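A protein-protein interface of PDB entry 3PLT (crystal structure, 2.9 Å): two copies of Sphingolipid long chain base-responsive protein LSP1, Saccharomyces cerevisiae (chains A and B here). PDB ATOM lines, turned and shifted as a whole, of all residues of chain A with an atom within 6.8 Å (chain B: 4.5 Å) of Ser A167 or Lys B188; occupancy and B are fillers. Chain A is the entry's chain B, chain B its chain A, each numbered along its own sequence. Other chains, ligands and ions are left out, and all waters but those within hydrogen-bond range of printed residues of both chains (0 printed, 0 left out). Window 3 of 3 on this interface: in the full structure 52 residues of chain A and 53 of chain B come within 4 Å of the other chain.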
ATOM      1  N   LYS A 161     -10.512  -1.252 -14.178  1.00  0.00           N
ATOM      2  CA  LYS A 161     -11.355  -2.052 -13.329  1.00  0.00           C
ATOM      3  C   LYS A 161     -12.599  -1.296 -12.872  1.00  0.00           C
ATOM      4  O   LYS A 161     -13.686  -1.851 -12.915  1.00  0.00           O
ATOM      5  CB  LYS A 161     -10.549  -2.654 -12.173  1.00  0.00           C
ATOM      6  CG  LYS A 161      -9.582  -3.734 -12.668  1.00  0.00           C
ATOM      7  CD  LYS A 161      -9.283  -4.801 -11.634  1.00  0.00           C
ATOM      8  CE  LYS A 161      -8.694  -6.071 -12.274  1.00  0.00           C
ATOM      9  NZ  LYS A 161      -9.733  -6.898 -12.955  1.00  0.00           N
ATOM     10  N   LEU A 162     -12.479  -0.036 -12.469  1.00  0.00           N
ATOM     11  CA  LEU A 162     -13.685   0.748 -12.157  1.00  0.00           C
ATOM     12  C   LEU A 162     -14.671   0.759 -13.330  1.00  0.00           C
ATOM     13  O   LEU A 162     -15.840   0.461 -13.161  1.00  0.00           O
ATOM     14  CB  LEU A 162     -13.329   2.185 -11.783  1.00  0.00           C
ATOM     15  CG  LEU A 162     -14.486   3.040 -11.259  1.00  0.00           C
ATOM     16  CD1 LEU A 162     -14.964   2.519  -9.912  1.00  0.00           C
ATOM     17  CD2 LEU A 162     -14.061   4.488 -11.145  1.00  0.00           C
ATOM     18  N   LYS A 163     -14.193   1.090 -14.522  1.00  0.00           N
ATOM     19  CA  LYS A 163     -15.053   1.092 -15.703  1.00  0.00           C
ATOM     20  C   LYS A 163     -15.679  -0.272 -15.912  1.00  0.00           C
ATOM     21  O   LYS A 163     -16.867  -0.360 -16.153  1.00  0.00           O
ATOM     22  CB  LYS A 163     -14.288   1.497 -16.967  1.00  0.00           C
ATOM     23  CG  LYS A 163     -15.147   1.506 -18.231  1.00  0.00           C
ATOM     24  CD  LYS A 163     -14.406   2.118 -19.427  1.00  0.00           C
ATOM     25  CE  LYS A 163     -15.324   2.305 -20.636  1.00  0.00           C
ATOM     26  NZ  LYS A 163     -14.596   2.901 -21.790  1.00  0.00           N
ATOM     27  N   ALA A 164     -14.877  -1.328 -15.829  1.00  0.00           N
ATOM     28  CA  ALA A 164     -15.376  -2.683 -16.041  1.00  0.00           C
ATOM     29  C   ALA A 164     -16.420  -2.997 -14.991  1.00  0.00           C
ATOM     30  O   ALA A 164     -17.553  -3.339 -15.314  1.00  0.00           O
ATOM     31  CB  ALA A 164     -14.248  -3.689 -15.963  1.00  0.00           C
ATOM     32  N   ALA A 165     -16.023  -2.869 -13.729  1.00  0.00           N
ATOM     33  CA  ALA A 165     -16.886  -3.180 -12.598  1.00  0.00           C
ATOM     34  C   ALA A 165     -18.294  -2.655 -12.812  1.00  0.00           C
ATOM     35  O   ALA A 165     -19.237  -3.440 -12.879  1.00  0.00           O
ATOM     36  CB  ALA A 165     -16.311  -2.601 -11.315  1.00  0.00           C
ATOM     37  N   TYR A 166     -18.437  -1.337 -12.936  1.00  0.00           N
ATOM     38  CA  TYR A 166     -19.760  -0.730 -13.005  1.00  0.00           C
ATOM     39  C   TYR A 166     -20.435  -0.968 -14.344  1.00  0.00           C
ATOM     40  O   TYR A 166     -21.634  -1.193 -14.396  1.00  0.00           O
ATOM     41  CB  TYR A 166     -19.695   0.760 -12.697  1.00  0.00           C
ATOM     42  CG  TYR A 166     -19.574   1.047 -11.225  1.00  0.00           C
ATOM     43  CD1 TYR A 166     -20.703   1.150 -10.413  1.00  0.00           C
ATOM     44  CD2 TYR A 166     -18.335   1.209 -10.641  1.00  0.00           C
ATOM     45  CE1 TYR A 166     -20.594   1.411  -9.050  1.00  0.00           C
ATOM     46  CE2 TYR A 166     -18.210   1.468  -9.276  1.00  0.00           C
ATOM     47  CZ  TYR A 166     -19.340   1.567  -8.486  1.00  0.00           C
ATOM     48  OH  TYR A 166     -19.178   1.832  -7.144  1.00  0.00           O
ATOM     49  N   SER A 167     -19.666  -0.924 -15.422  1.00  0.00           N
ATOM     50  CA  SER A 167     -20.185  -1.287 -16.725  1.00  0.00           C
ATOM     51  C   SER A 167     -20.889  -2.629 -16.624  1.00  0.00           C
ATOM     52  O   SER A 167     -22.055  -2.750 -16.978  1.00  0.00           O
ATOM     53  CB  SER A 167     -19.063  -1.379 -17.754  1.00  0.00           C
ATOM     54  OG  SER A 167     -19.498  -2.092 -18.900  1.00  0.00           O
ATOM     55  N   TYR A 168     -20.175  -3.632 -16.129  1.00  0.00           N
ATOM     56  CA  TYR A 168     -20.725  -4.964 -16.002  1.00  0.00           C
ATOM     57  C   TYR A 168     -21.965  -4.876 -15.134  1.00  0.00           C
ATOM     58  O   TYR A 168     -23.072  -5.214 -15.563  1.00  0.00           O
ATOM     59  CB  TYR A 168     -19.685  -5.915 -15.402  1.00  0.00           C
ATOM     60  CG  TYR A 168     -20.090  -7.383 -15.362  1.00  0.00           C
ATOM     61  CD1 TYR A 168     -20.568  -8.041 -16.509  1.00  0.00           C
ATOM     62  CD2 TYR A 168     -19.964  -8.135 -14.172  1.00  0.00           C
ATOM     63  CE1 TYR A 168     -20.934  -9.401 -16.474  1.00  0.00           C
ATOM     64  CE2 TYR A 168     -20.320  -9.503 -14.129  1.00  0.00           C
ATOM     65  CZ  TYR A 168     -20.805 -10.125 -15.286  1.00  0.00           C
ATOM     66  OH  TYR A 168     -21.162 -11.459 -15.249  1.00  0.00           O
ATOM     67  N   MET A 169     -21.794  -4.364 -13.929  1.00  0.00           N
ATOM     68  CA  MET A 169     -22.880  -4.357 -12.969  1.00  0.00           C
ATOM     69  C   MET A 169     -24.171  -3.810 -13.567  1.00  0.00           C
ATOM     70  O   MET A 169     -25.216  -4.424 -13.423  1.00  0.00           O
ATOM     71  CB  MET A 169     -22.481  -3.567 -11.733  1.00  0.00           C
ATOM     72  CG  MET A 169     -23.499  -3.592 -10.624  1.00  0.00           C
ATOM     73  SD  MET A 169     -24.755  -2.347 -10.888  1.00  0.00           S
ATOM     74  CE  MET A 169     -23.880  -0.823 -10.573  1.00  0.00           C
ATOM     75  N   PHE A 170     -24.095  -2.678 -14.258  1.00  0.00           N
ATOM     76  CA  PHE A 170     -25.291  -2.029 -14.798  1.00  0.00           C
ATOM     77  C   PHE A 170     -26.022  -2.807 -15.875  1.00  0.00           C
ATOM     78  O   PHE A 170     -27.255  -2.823 -15.892  1.00  0.00           O
ATOM     79  CB  PHE A 170     -24.963  -0.646 -15.354  1.00  0.00           C
ATOM     80  CG  PHE A 170     -24.792   0.401 -14.299  1.00  0.00           C
ATOM     81  CD1 PHE A 170     -25.676   0.495 -13.234  1.00  0.00           C
ATOM     82  CD2 PHE A 170     -23.757   1.306 -14.378  1.00  0.00           C
ATOM     83  CE1 PHE A 170     -25.519   1.465 -12.267  1.00  0.00           C
ATOM     84  CE2 PHE A 170     -23.595   2.273 -13.408  1.00  0.00           C
ATOM     85  CZ  PHE A 170     -24.481   2.351 -12.350  1.00  0.00           C
ATOM     86  N   ASP A 171     -25.280  -3.424 -16.787  1.00  0.00           N
ATOM     87  CA  ASP A 171     -25.894  -4.280 -17.792  1.00  0.00           C
ATOM     88  C   ASP A 171     -26.670  -5.402 -17.108  1.00  0.00           C
ATOM     89  O   ASP A 171     -27.800  -5.696 -17.478  1.00  0.00           O
ATOM     90  CB  ASP A 171     -24.836  -4.870 -18.720  1.00  0.00           C
ATOM     91  CG  ASP A 171     -24.217  -3.828 -19.659  1.00  0.00           C
ATOM     92  OD1 ASP A 171     -24.851  -2.779 -19.932  1.00  0.00           O
ATOM     93  OD2 ASP A 171     -23.089  -4.075 -20.141  1.00  0.00           O
ATOM     94  N   SER A 172     -26.061  -6.013 -16.095  1.00  0.00           N
ATOM     95  CA  SER A 172     -26.731  -7.045 -15.308  1.00  0.00           C
ATOM     96  C   SER A 172     -27.972  -6.509 -14.611  1.00  0.00           C
ATOM     97  O   SER A 172     -28.976  -7.198 -14.534  1.00  0.00           O
ATOM     98  CB  SER A 172     -25.786  -7.638 -14.259  1.00  0.00           C
ATOM     99  OG  SER A 172     -24.538  -7.955 -14.829  1.00  0.00           O
ATOM    100  N   ARG A 174     -29.702  -3.862 -15.643  1.00  0.00           N
ATOM    101  CA  ARG A 174     -30.656  -3.641 -16.712  1.00  0.00           C
ATOM    102  C   ARG A 174     -31.326  -4.954 -17.129  1.00  0.00           C
ATOM    103  O   ARG A 174     -32.511  -4.970 -17.442  1.00  0.00           O
ATOM    104  CB  ARG A 174     -30.021  -2.938 -17.912  1.00  0.00           C
ATOM    105  CG  ARG A 174     -31.023  -2.671 -19.050  1.00  0.00           C
ATOM    106  CD  ARG A 174     -30.745  -1.395 -19.798  1.00  0.00           C
ATOM    107  NE  ARG A 174     -29.476  -1.466 -20.517  1.00  0.00           N
ATOM    108  CZ  ARG A 174     -29.308  -2.004 -21.727  1.00  0.00           C
ATOM    109  NH1 ARG A 174     -30.334  -2.541 -22.392  1.00  0.00           N
ATOM    110  NH2 ARG A 174     -28.097  -2.004 -22.282  1.00  0.00           N
ATOM    111  N   LEU A 230     -29.743  -7.682 -24.576  1.00  0.00           N
ATOM    112  CA  LEU A 230     -29.254  -6.316 -24.563  1.00  0.00           C
ATOM    113  C   LEU A 230     -29.135  -5.892 -26.016  1.00  0.00           C
ATOM    114  O   LEU A 230     -28.945  -6.742 -26.896  1.00  0.00           O
ATOM    115  CB  LEU A 230     -27.870  -6.251 -23.925  1.00  0.00           C
ATOM    116  CG  LEU A 230     -27.715  -6.512 -22.433  1.00  0.00           C
ATOM    117  CD1 LEU A 230     -26.275  -6.893 -22.120  1.00  0.00           C
ATOM    118  CD2 LEU A 230     -28.133  -5.284 -21.645  1.00  0.00           C
ATOM    119  N   ALA B 184     -29.945   2.338 -15.047  1.00  0.00           N
ATOM    120  CA  ALA B 184     -28.871   1.486 -15.544  1.00  0.00           C
ATOM    121  C   ALA B 184     -28.368   2.031 -16.866  1.00  0.00           C
ATOM    122  O   ALA B 184     -27.183   2.320 -17.005  1.00  0.00           O
ATOM    123  CB  ALA B 184     -29.343   0.072 -15.719  1.00  0.00           C
ATOM    124  N   GLY B 185     -29.277   2.187 -17.826  1.00  0.00           N
ATOM    125  CA  GLY B 185     -28.921   2.655 -19.163  1.00  0.00           C
ATOM    126  C   GLY B 185     -28.204   3.991 -19.149  1.00  0.00           C
ATOM    127  O   GLY B 185     -27.231   4.180 -19.869  1.00  0.00           O
ATOM    128  N   TYR B 186     -28.685   4.923 -18.333  1.00  0.00           N
ATOM    129  CA  TYR B 186     -28.040   6.227 -18.205  1.00  0.00           C
ATOM    130  C   TYR B 186     -26.758   6.093 -17.394  1.00  0.00           C
ATOM    131  O   TYR B 186     -25.741   6.690 -17.728  1.00  0.00           O
ATOM    132  CB  TYR B 186     -28.990   7.269 -17.590  1.00  0.00           C
ATOM    133  CG  TYR B 186     -30.027   7.786 -18.577  1.00  0.00           C
ATOM    134  CD1 TYR B 186     -29.641   8.484 -19.719  1.00  0.00           C
ATOM    135  CD2 TYR B 186     -31.377   7.585 -18.376  1.00  0.00           C
ATOM    136  CE1 TYR B 186     -30.572   8.954 -20.630  1.00  0.00           C
ATOM    137  CE2 TYR B 186     -32.319   8.059 -19.286  1.00  0.00           C
ATOM    138  CZ  TYR B 186     -31.905   8.738 -20.408  1.00  0.00           C
ATOM    139  OH  TYR B 186     -32.824   9.203 -21.311  1.00  0.00           O
ATOM    140  N   GLY B 187     -26.795   5.286 -16.346  1.00  0.00           N
ATOM    141  CA  GLY B 187     -25.600   5.008 -15.575  1.00  0.00           C
ATOM    142  C   GLY B 187     -24.459   4.526 -16.450  1.00  0.00           C
ATOM    143  O   GLY B 187     -23.312   4.884 -16.219  1.00  0.00           O
ATOM    144  N   LYS B 188     -24.764   3.713 -17.459  1.00  0.00           N
ATOM    145  CA  LYS B 188     -23.726   3.188 -18.340  1.00  0.00           C
ATOM    146  C   LYS B 188     -23.280   4.238 -19.341  1.00  0.00           C
ATOM    147  O   LYS B 188     -22.162   4.199 -19.846  1.00  0.00           O
ATOM    148  CB  LYS B 188     -24.193   1.934 -19.070  1.00  0.00           C
ATOM    149  CG  LYS B 188     -23.059   1.251 -19.803  1.00  0.00           C
ATOM    150  CD  LYS B 188     -23.312  -0.221 -20.068  1.00  0.00           C
ATOM    151  CE  LYS B 188     -22.153  -0.832 -20.884  1.00  0.00           C
ATOM    152  NZ  LYS B 188     -22.583  -2.013 -21.711  1.00  0.00           N
ATOM    153  N   ALA B 189     -24.160   5.186 -19.624  1.00  0.00           N
ATOM    154  CA  ALA B 189     -23.821   6.300 -20.493  1.00  0.00           C
ATOM    155  C   ALA B 189     -22.781   7.205 -19.853  1.00  0.00           C
ATOM    156  O   ALA B 189     -22.040   7.857 -20.570  1.00  0.00           O
ATOM    157  CB  ALA B 189     -25.060   7.088 -20.839  1.00  0.00           C
ATOM    158  N   LEU B 190     -22.736   7.253 -18.521  1.00  0.00           N
ATOM    159  CA  LEU B 190     -21.690   7.994 -17.797  1.00  0.00           C
ATOM    160  C   LEU B 190     -20.329   7.329 -17.931  1.00  0.00           C
ATOM    161  O   LEU B 190     -19.325   7.996 -18.129  1.00  0.00           O
ATOM    162  CB  LEU B 190     -22.026   8.121 -16.309  1.00  0.00           C
ATOM    163  CG  LEU B 190     -22.834   9.353 -15.917  1.00  0.00           C
ATOM    164  CD1 LEU B 190     -23.526   9.153 -14.575  1.00  0.00           C
ATOM    165  CD2 LEU B 190     -21.939  10.575 -15.887  1.00  0.00           C
ATOM    166  N   LEU B 191     -20.292   6.012 -17.811  1.00  0.00           N
ATOM    167  CA  LEU B 191     -19.034   5.293 -17.909  1.00  0.00           C
ATOM    168  C   LEU B 191     -18.344   5.503 -19.256  1.00  0.00           C
ATOM    169  O   LEU B 191     -17.130   5.311 -19.348  1.00  0.00           O
ATOM    170  CB  LEU B 191     -19.235   3.795 -17.666  1.00  0.00           C
ATOM    171  CG  LEU B 191     -19.697   3.389 -16.263  1.00  0.00           C
ATOM    172  CD1 LEU B 191     -19.937   1.889 -16.167  1.00  0.00           C
ATOM    173  CD2 LEU B 191     -18.683   3.843 -15.218  1.00  0.00           C
ATOM    174  N   GLU B 192     -19.089   5.877 -20.298  1.00  0.00           N
ATOM    175  CA  GLU B 192     -18.452   6.243 -21.573  1.00  0.00           C
ATOM    176  C   GLU B 192     -17.517   7.454 -21.421  1.00  0.00           C
ATOM    177  O   GLU B 192     -16.492   7.520 -22.094  1.00  0.00           O
ATOM    178  CB  GLU B 192     -19.478   6.502 -22.687  1.00  0.00           C
ATOM    179  CG  GLU B 192     -19.897   5.238 -23.493  1.00  0.00           C
ATOM    180  CD  GLU B 192     -20.382   5.566 -24.933  1.00  0.00           C
ATOM    181  OE1 GLU B 192     -19.610   5.312 -25.895  1.00  0.00           O
ATOM    182  OE2 GLU B 192     -21.521   6.085 -25.098  1.00  0.00           O
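Among the printed residues, merely in contact across the chains: Ser A167 with Leu B191 (2.9 Å), Tyr A166 with Leu B191 (3.4 Å), Ser A167 with Lys B188 (3.5 Å), Phe A170 with Ala B184 (3.6 Å), Lys A163 with Leu B191 (3.7 Å), Arg A174 with Ala B184 (3.8 Å) and Phe A170 with Gly B187 (3.8 Å).
Hydrophobic or aromatic side chains of chain B within 4 Å of the printed part of chain A: Ala B184 and Leu B191. Of the 14 printed residues of chain A, 6 touch a printed residue of chain B. Among the printed residues, 8 pairs touch across the chains. Among the printed residues, Asp or Glu carboxylates within 4 Å of a Lys or Arg side-chain nitrogen of the other chain: Asp A171 with Lys B188 (2.6 Å).
Ser A167 touches two residues of chain B. Lys B188 touches two residues of chain A. Printed residues of chain B within 4 Å of Lys A163: Leu B191 (3.7 Å). Of the printed residues of chain B, Arg A174 touches Ala B184 (3.8 Å). The nearest printed residue of chain B that does not touch Ser A167 is Gly B187 (6.9 Å).
The side-chain amino group (NZ) of Lys B188 is in salt-bridge range of the side-chain carboxylate (OD2) of Asp A171, at 2.6 Å.
No position is printed for both chains.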
